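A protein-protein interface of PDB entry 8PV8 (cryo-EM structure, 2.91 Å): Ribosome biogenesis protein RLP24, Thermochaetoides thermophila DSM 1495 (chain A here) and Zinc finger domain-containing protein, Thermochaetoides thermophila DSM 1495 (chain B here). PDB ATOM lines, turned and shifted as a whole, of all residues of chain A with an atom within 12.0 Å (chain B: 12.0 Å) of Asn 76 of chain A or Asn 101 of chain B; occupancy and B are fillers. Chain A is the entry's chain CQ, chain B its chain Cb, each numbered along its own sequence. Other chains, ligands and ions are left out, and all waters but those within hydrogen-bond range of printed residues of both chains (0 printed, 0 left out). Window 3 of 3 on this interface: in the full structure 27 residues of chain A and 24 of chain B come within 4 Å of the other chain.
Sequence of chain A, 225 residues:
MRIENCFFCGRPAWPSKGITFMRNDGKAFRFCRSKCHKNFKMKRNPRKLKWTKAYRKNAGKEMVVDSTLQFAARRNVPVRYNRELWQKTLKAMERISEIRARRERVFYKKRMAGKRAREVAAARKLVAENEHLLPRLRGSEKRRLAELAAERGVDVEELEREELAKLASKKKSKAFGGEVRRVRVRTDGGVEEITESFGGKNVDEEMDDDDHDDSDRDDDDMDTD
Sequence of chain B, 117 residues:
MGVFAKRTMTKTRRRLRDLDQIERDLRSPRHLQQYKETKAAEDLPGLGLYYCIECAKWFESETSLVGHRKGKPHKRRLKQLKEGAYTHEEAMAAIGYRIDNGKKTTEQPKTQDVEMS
Along chain A the printed residues that touch a printed residue of chain B span positions 2 to 77. Among the printed residues, Asp or Glu carboxylates within 4 Å of a Lys or Arg side-chain nitrogen of the other chain: Arg 75 of chain A with Asp 100 of chain B (3.3 Å).
Asn 76 of chain A touches just these residues of chain B: Ile 99 (3.4 Å), Asp 100 (2.9 Å) and Asn 101 (2.8 Å). Asn 101 of chain B touches just these residues of chain A: Asn 76 and Val 77. Of the printed residues of chain B, Arg 74 of chain A touches Tyr 97, Arg 98, Ile 99 and Asp 100. Of chain B, only Asn 101 (3.4 Å) comes within 4 Å of Val 77 of chain A. No residue of chain B comes within 4 Å of Pro 78 of chain A. Ile 99 of chain B touches just these residues of chain A: Arg 74 (3.7 Å) and Asn 76 (3.4 Å). No residue of chain A comes within 4 Å of Gly 102 of chain B. Of the printed residues of chain A, Tyr 97 of chain B touches Arg 2 (3.4 Å), Ala 73 (3.6 Å) and Arg 74 (3.3 Å). Of the printed residues of chain B, Arg 75 of chain A touches Asp 100. Arg 80 of chain A touches none of the printed residues of chain B. The nearest residue of chain B that does not touch Asn 76 of chain A is Gly 102 of chain B (6.0 Å). The nearest residue of chain A that does not touch Asn 101 of chain B is Arg 74 of chain A (5.0 Å).
O of Met 92 of chain B sits at hydrogen-bond distance from N of Tyr 97 of chain B, 2.8 Å away. OD1 of Asp 100 of chain B lies within hydrogen-bond range of N of Gly 102 of chain B, 3.2 Å away. NE of Arg 2 of chain A is in salt-bridge range of OE1 of Glu 4 of chain A. The backbone carbonyl oxygen (O) of Phe 71 of chain A sits at hydrogen-bond distance from the guanidinium group (NH2) of Arg 75 of chain A (2.5 Å). NH1 of Arg 74 of chain A is in hydrogen-bond range of OD1 of Asn 76 of chain A (3.2 Å).
Among the printed residues, merely in contact across the chains: Ala 73 of chain A with Arg 98 of chain B, Val 77 of chain A with Asn 101 of chain B, Asn 76 of chain A with Ile 99 of chain B, Ala 73 of chain A with Tyr 97 of chain B, Arg 74 of chain A with Ile 99 of chain B, Ala 73 of chain A with Asp 100 of chain B and Ala 72 of chain A with Arg 98 of chain B.
OH of Tyr 97 of chain B is in hydrogen-bond range of NH2 of Arg 2 of chain A (3.4 Å). The side-chain hydroxyl of Tyr 97 of chain B lies close to the backbone NH of Arg 74 of chain A, at 3.3 Å. The backbone carbonyl oxygen of Gln 70 of chain A sits at hydrogen-bond distance from the guanidinium group of Arg 98 of chain B (3.0 Å). The backbone carbonyl oxygen (O) of Arg 98 of chain B sits at hydrogen-bond distance from the backbone NH (N) of Arg 74 of chain A, 3.0 Å away. The backbone NH (N) of Asp 100 of chain B is in hydrogen-bond range of the backbone carbonyl oxygen (O) of Arg 74 of chain A. NH1 of Arg 75 of chain A lies within salt-bridge range of OD2 of Asp 100 of chain B (3.3 Å). O of Asp 100 of chain B lies within hydrogen-bond range of N of Asn 76 of chain A, 2.9 Å away. OD1 of Asn 101 of chain B is in hydrogen-bond range of ND2 of Asn 76 of chain A (2.8 Å).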
ATOM      1  N   ARG A   2      21.123 -12.207 -22.972  1.00  0.00           N
ATOM      2  CA  ARG A   2      20.233 -13.255 -22.498  1.00  0.00           C
ATOM      3  C   ARG A   2      20.348 -14.467 -23.409  1.00  0.00           C
ATOM      4  O   ARG A   2      20.942 -14.408 -24.488  1.00  0.00           O
ATOM      5  CB  ARG A   2      18.778 -12.772 -22.444  1.00  0.00           C
ATOM      6  CG  ARG A   2      18.163 -12.540 -23.814  1.00  0.00           C
ATOM      7  CD  ARG A   2      16.662 -12.295 -23.741  1.00  0.00           C
ATOM      8  NE  ARG A   2      15.908 -13.489 -23.377  1.00  0.00           N
ATOM      9  CZ  ARG A   2      15.410 -13.723 -22.170  1.00  0.00           C
ATOM     10  NH1 ARG A   2      15.572 -12.865 -21.177  1.00  0.00           N
ATOM     11  NH2 ARG A   2      14.731 -14.845 -21.956  1.00  0.00           N
ATOM     12  N   GLU A   4      18.405 -16.933 -25.689  1.00  0.00           N
ATOM     13  CA  GLU A   4      17.167 -17.150 -26.415  1.00  0.00           C
ATOM     14  C   GLU A   4      16.979 -18.646 -26.645  1.00  0.00           C
ATOM     15  O   GLU A   4      17.798 -19.470 -26.240  1.00  0.00           O
ATOM     16  CB  GLU A   4      17.179 -16.383 -27.736  1.00  0.00           C
ATOM     17  CG  GLU A   4      17.600 -14.927 -27.617  1.00  0.00           C
ATOM     18  CD  GLU A   4      16.440 -13.994 -27.323  1.00  0.00           C
ATOM     19  OE1 GLU A   4      15.321 -14.486 -27.066  1.00  0.00           O
ATOM     20  OE2 GLU A   4      16.648 -12.763 -27.349  1.00  0.00           O
ATOM     21  N   GLN A  70       7.359 -23.856 -13.636  1.00  0.00           N
ATOM     22  CA  GLN A  70       6.570 -22.646 -13.455  1.00  0.00           C
ATOM     23  C   GLN A  70       7.395 -21.494 -12.895  1.00  0.00           C
ATOM     24  O   GLN A  70       6.837 -20.443 -12.562  1.00  0.00           O
ATOM     25  CB  GLN A  70       5.371 -22.933 -12.551  1.00  0.00           C
ATOM     26  CG  GLN A  70       4.491 -24.065 -13.049  1.00  0.00           C
ATOM     27  CD  GLN A  70       3.948 -23.812 -14.439  1.00  0.00           C
ATOM     28  OE1 GLN A  70       4.357 -24.459 -15.404  1.00  0.00           O
ATOM     29  NE2 GLN A  70       3.021 -22.869 -14.552  1.00  0.00           N
ATOM     30  N   PHE A  71       8.711 -21.671 -12.785  1.00  0.00           N
ATOM     31  CA  PHE A  71       9.588 -20.657 -12.217  1.00  0.00           C
ATOM     32  C   PHE A  71      10.263 -19.786 -13.266  1.00  0.00           C
ATOM     33  O   PHE A  71      10.635 -18.650 -12.955  1.00  0.00           O
ATOM     34  CB  PHE A  71      10.663 -21.320 -11.351  1.00  0.00           C
ATOM     35  CG  PHE A  71      10.116 -22.044 -10.160  1.00  0.00           C
ATOM     36  CD1 PHE A  71       9.827 -21.361  -8.991  1.00  0.00           C
ATOM     37  CD2 PHE A  71       9.903 -23.412 -10.202  1.00  0.00           C
ATOM     38  CE1 PHE A  71       9.332 -22.029  -7.891  1.00  0.00           C
ATOM     39  CE2 PHE A  71       9.405 -24.084  -9.103  1.00  0.00           C
ATOM     40  CZ  PHE A  71       9.118 -23.390  -7.946  1.00  0.00           C
ATOM     41  N   ALA A  72      10.434 -20.284 -14.487  1.00  0.00           N
ATOM     42  CA  ALA A  72      11.064 -19.533 -15.563  1.00  0.00           C
ATOM     43  C   ALA A  72       9.989 -18.981 -16.486  1.00  0.00           C
ATOM     44  O   ALA A  72       9.183 -19.742 -17.031  1.00  0.00           O
ATOM     45  CB  ALA A  72      12.039 -20.412 -16.349  1.00  0.00           C
ATOM     46  N   ALA A  73       9.981 -17.662 -16.659  1.00  0.00           N
ATOM     47  CA  ALA A  73       8.981 -17.012 -17.492  1.00  0.00           C
ATOM     48  C   ALA A  73       9.543 -15.695 -17.999  1.00  0.00           C
ATOM     49  O   ALA A  73      10.475 -15.133 -17.421  1.00  0.00           O
ATOM     50  CB  ALA A  73       7.676 -16.779 -16.725  1.00  0.00           C
ATOM     51  N   ARG A  74       8.958 -15.208 -19.089  1.00  0.00           N
ATOM     52  CA  ARG A  74       9.324 -13.904 -19.637  1.00  0.00           C
ATOM     53  C   ARG A  74       8.586 -12.839 -18.841  1.00  0.00           C
ATOM     54  O   ARG A  74       7.432 -12.516 -19.128  1.00  0.00           O
ATOM     55  CB  ARG A  74       8.992 -13.827 -21.122  1.00  0.00           C
ATOM     56  CG  ARG A  74       9.553 -12.603 -21.824  1.00  0.00           C
ATOM     57  CD  ARG A  74       9.344 -12.690 -23.328  1.00  0.00           C
ATOM     58  NE  ARG A  74      10.204 -11.767 -24.058  1.00  0.00           N
ATOM     59  CZ  ARG A  74       9.840 -10.552 -24.444  1.00  0.00           C
ATOM     60  NH1 ARG A  74       8.628 -10.083 -24.196  1.00  0.00           N
ATOM     61  NH2 ARG A  74      10.713  -9.789 -25.095  1.00  0.00           N
ATOM     62  N   ARG A  75       9.253 -12.298 -17.826  1.00  0.00           N
ATOM     63  CA  ARG A  75       8.647 -11.300 -16.957  1.00  0.00           C
ATOM     64  C   ARG A  75       8.552  -9.974 -17.701  1.00  0.00           C
ATOM     65  O   ARG A  75       9.572  -9.330 -17.968  1.00  0.00           O
ATOM     66  CB  ARG A  75       9.463 -11.149 -15.678  1.00  0.00           C
ATOM     67  CG  ARG A  75      10.020 -12.460 -15.154  1.00  0.00           C
ATOM     68  CD  ARG A  75       8.932 -13.311 -14.529  1.00  0.00           C
ATOM     69  NE  ARG A  75       9.458 -14.559 -13.991  1.00  0.00           N
ATOM     70  CZ  ARG A  75       8.739 -15.441 -13.311  1.00  0.00           C
ATOM     71  NH1 ARG A  75       7.457 -15.238 -13.057  1.00  0.00           N
ATOM     72  NH2 ARG A  75       9.321 -16.555 -12.877  1.00  0.00           N
ATOM     73  N   ASN A  76       7.327  -9.569 -18.035  1.00  0.00           N
ATOM     74  CA  ASN A  76       7.090  -8.324 -18.747  1.00  0.00           C
ATOM     75  C   ASN A  76       6.862  -7.137 -17.826  1.00  0.00           C
ATOM     76  O   ASN A  76       6.796  -6.003 -18.312  1.00  0.00           O
ATOM     77  CB  ASN A  76       5.886  -8.472 -19.687  1.00  0.00           C
ATOM     78  CG  ASN A  76       6.236  -9.194 -20.971  1.00  0.00           C
ATOM     79  OD1 ASN A  76       7.378  -9.153 -21.428  1.00  0.00           O
ATOM     80  ND2 ASN A  76       5.251  -9.848 -21.569  1.00  0.00           N
ATOM     81  N   VAL A  77       6.741  -7.364 -16.523  1.00  0.00           N
ATOM     82  CA  VAL A  77       6.654  -6.307 -15.524  1.00  0.00           C
ATOM     83  C   VAL A  77       7.950  -6.341 -14.716  1.00  0.00           C
ATOM     84  O   VAL A  77       8.173  -7.291 -13.950  1.00  0.00           O
ATOM     85  CB  VAL A  77       5.425  -6.476 -14.621  1.00  0.00           C
ATOM     86  CG1 VAL A  77       5.384  -5.380 -13.571  1.00  0.00           C
ATOM     87  CG2 VAL A  77       4.156  -6.466 -15.455  1.00  0.00           C
ATOM     88  N   PRO A  78       8.832  -5.357 -14.863  1.00  0.00           N
ATOM     89  CA  PRO A  78      10.128  -5.413 -14.182  1.00  0.00           C
ATOM     90  C   PRO A  78      10.000  -5.224 -12.679  1.00  0.00           C
ATOM     91  O   PRO A  78       9.040  -4.645 -12.166  1.00  0.00           O
ATOM     92  CB  PRO A  78      10.908  -4.258 -14.817  1.00  0.00           C
ATOM     93  CG  PRO A  78       9.852  -3.305 -15.247  1.00  0.00           C
ATOM     94  CD  PRO A  78       8.716  -4.164 -15.717  1.00  0.00           C
ATOM     95  N   VAL A  79      11.004  -5.737 -11.975  1.00  0.00           N
ATOM     96  CA  VAL A  79      11.115  -5.625 -10.528  1.00  0.00           C
ATOM     97  C   VAL A  79      12.326  -4.759 -10.219  1.00  0.00           C
ATOM     98  O   VAL A  79      13.386  -4.927 -10.833  1.00  0.00           O
ATOM     99  CB  VAL A  79      11.239  -7.016  -9.868  1.00  0.00           C
ATOM    100  CG1 VAL A  79      11.459  -6.898  -8.365  1.00  0.00           C
ATOM    101  CG2 VAL A  79      10.010  -7.856 -10.168  1.00  0.00           C
ATOM    102  N   ARG A  80      12.154  -3.809  -9.298  1.00  0.00           N
ATOM    103  CA  ARG A  80      13.253  -2.959  -8.858  1.00  0.00           C
ATOM    104  C   ARG A  80      14.360  -3.804  -8.235  1.00  0.00           C
ATOM    105  O   ARG A  80      14.099  -4.806  -7.563  1.00  0.00           O
ATOM    106  CB  ARG A  80      12.737  -1.925  -7.855  1.00  0.00           C
ATOM    107  CG  ARG A  80      13.762  -0.915  -7.373  1.00  0.00           C
ATOM    108  CD  ARG A  80      13.090   0.191  -6.588  1.00  0.00           C
ATOM    109  NE  ARG A  80      11.992   0.786  -7.338  1.00  0.00           N
ATOM    110  CZ  ARG A  80      12.131   1.781  -8.204  1.00  0.00           C
ATOM    111  NH1 ARG A  80      13.310   2.326  -8.448  1.00  0.00           N
ATOM    112  NH2 ARG A  80      11.057   2.239  -8.841  1.00  0.00           N
ATOM    113  N   GLU B  89       3.805 -19.758 -29.973  1.00  0.00           N
ATOM    114  CA  GLU B  89       3.195 -20.279 -28.754  1.00  0.00           C
ATOM    115  C   GLU B  89       3.444 -21.775 -28.615  1.00  0.00           C
ATOM    116  O   GLU B  89       3.699 -22.273 -27.513  1.00  0.00           O
ATOM    117  CB  GLU B  89       1.696 -19.978 -28.746  1.00  0.00           C
ATOM    118  CG  GLU B  89       1.354 -18.500 -28.836  1.00  0.00           C
ATOM    119  CD  GLU B  89       0.943 -18.081 -30.233  1.00  0.00           C
ATOM    120  OE1 GLU B  89       0.252 -17.050 -30.367  1.00  0.00           O
ATOM    121  OE2 GLU B  89       1.303 -18.787 -31.197  1.00  0.00           O
ATOM    122  N   MET B  92       7.068 -22.166 -27.446  1.00  0.00           N
ATOM    123  CA  MET B  92       7.178 -21.940 -26.006  1.00  0.00           C
ATOM    124  C   MET B  92       6.569 -23.086 -25.207  1.00  0.00           C
ATOM    125  O   MET B  92       7.075 -23.438 -24.137  1.00  0.00           O
ATOM    126  CB  MET B  92       6.528 -20.611 -25.632  1.00  0.00           C
ATOM    127  CG  MET B  92       7.021 -19.439 -26.447  1.00  0.00           C
ATOM    128  SD  MET B  92       7.053 -17.902 -25.528  1.00  0.00           S
ATOM    129  CE  MET B  92       5.348 -17.422 -25.767  1.00  0.00           C
ATOM    130  N   TYR B  97       8.088 -22.828 -21.619  1.00  0.00           N
ATOM    131  CA  TYR B  97       8.360 -21.439 -21.282  1.00  0.00           C
ATOM    132  C   TYR B  97       7.074 -20.646 -21.476  1.00  0.00           C
ATOM    133  O   TYR B  97       6.312 -20.921 -22.407  1.00  0.00           O
ATOM    134  CB  TYR B  97       9.489 -20.907 -22.167  1.00  0.00           C
ATOM    135  CG  TYR B  97      10.030 -19.542 -21.829  1.00  0.00           C
ATOM    136  CD1 TYR B  97      10.865 -19.365 -20.735  1.00  0.00           C
ATOM    137  CD2 TYR B  97       9.758 -18.445 -22.634  1.00  0.00           C
ATOM    138  CE1 TYR B  97      11.384 -18.132 -20.431  1.00  0.00           C
ATOM    139  CE2 TYR B  97      10.276 -17.203 -22.337  1.00  0.00           C
ATOM    140  CZ  TYR B  97      11.088 -17.055 -21.234  1.00  0.00           C
ATOM    141  OH  TYR B  97      11.614 -15.825 -20.928  1.00  0.00           O
ATOM    142  N   ARG B  98       6.816 -19.686 -20.592  1.00  0.00           N
ATOM    143  CA  ARG B  98       5.533 -18.997 -20.555  1.00  0.00           C
ATOM    144  C   ARG B  98       5.735 -17.497 -20.407  1.00  0.00           C
ATOM    145  O   ARG B  98       6.784 -17.051 -19.935  1.00  0.00           O
ATOM    146  CB  ARG B  98       4.661 -19.534 -19.415  1.00  0.00           C
ATOM    147  CG  ARG B  98       5.407 -19.777 -18.114  1.00  0.00           C
ATOM    148  CD  ARG B  98       4.448 -20.124 -16.988  1.00  0.00           C
ATOM    149  NE  ARG B  98       3.950 -18.939 -16.301  1.00  0.00           N
ATOM    150  CZ  ARG B  98       4.576 -18.338 -15.298  1.00  0.00           C
ATOM    151  NH1 ARG B  98       5.719 -18.801 -14.822  1.00  0.00           N
ATOM    152  NH2 ARG B  98       4.037 -17.251 -14.755  1.00  0.00           N
ATOM    153  N   ILE B  99       4.734 -16.725 -20.832  1.00  0.00           N
ATOM    154  CA  ILE B  99       4.779 -15.276 -20.681  1.00  0.00           C
ATOM    155  C   ILE B  99       4.132 -14.879 -19.363  1.00  0.00           C
ATOM    156  O   ILE B  99       3.015 -15.309 -19.042  1.00  0.00           O
ATOM    157  CB  ILE B  99       4.076 -14.589 -21.864  1.00  0.00           C
ATOM    158  CG1 ILE B  99       4.705 -15.009 -23.185  1.00  0.00           C
ATOM    159  CG2 ILE B  99       4.151 -13.085 -21.729  1.00  0.00           C
ATOM    160  CD1 ILE B  99       6.160 -14.652 -23.320  1.00  0.00           C
ATOM    161  N   ASP B 100       4.830 -14.055 -18.586  1.00  0.00           N
ATOM    162  CA  ASP B 100       4.305 -13.515 -17.338  1.00  0.00           C
ATOM    163  C   ASP B 100       4.023 -12.031 -17.527  1.00  0.00           C
ATOM    164  O   ASP B 100       4.954 -11.223 -17.596  1.00  0.00           O
ATOM    165  CB  ASP B 100       5.287 -13.737 -16.188  1.00  0.00           C
ATOM    166  CG  ASP B 100       4.805 -13.134 -14.881  1.00  0.00           C
ATOM    167  OD1 ASP B 100       3.577 -13.100 -14.653  1.00  0.00           O
ATOM    168  OD2 ASP B 100       5.655 -12.694 -14.079  1.00  0.00           O
ATOM    169  N   ASN B 101       2.742 -11.678 -17.609  1.00  0.00           N
ATOM    170  CA  ASN B 101       2.316 -10.293 -17.758  1.00  0.00           C
ATOM    171  C   ASN B 101       1.949  -9.634 -16.436  1.00  0.00           C
ATOM    172  O   ASN B 101       1.558  -8.463 -16.433  1.00  0.00           O
ATOM    173  CB  ASN B 101       1.125 -10.206 -18.718  1.00  0.00           C
ATOM    174  CG  ASN B 101       1.505 -10.537 -20.145  1.00  0.00           C
ATOM    175  OD1 ASN B 101       2.669 -10.435 -20.527  1.00  0.00           O
ATOM    176  ND2 ASN B 101       0.522 -10.938 -20.944  1.00  0.00           N
ATOM    177  N   GLY B 102       2.065 -10.346 -15.321  1.00  0.00           N
ATOM    178  CA  GLY B 102       1.735  -9.787 -14.023  1.00  0.00           C
ATOM    179  C   GLY B 102       0.245  -9.637 -13.795  1.00  0.00           C
ATOM    180  O   GLY B 102      -0.565 -10.152 -14.565  1.00  0.00           O
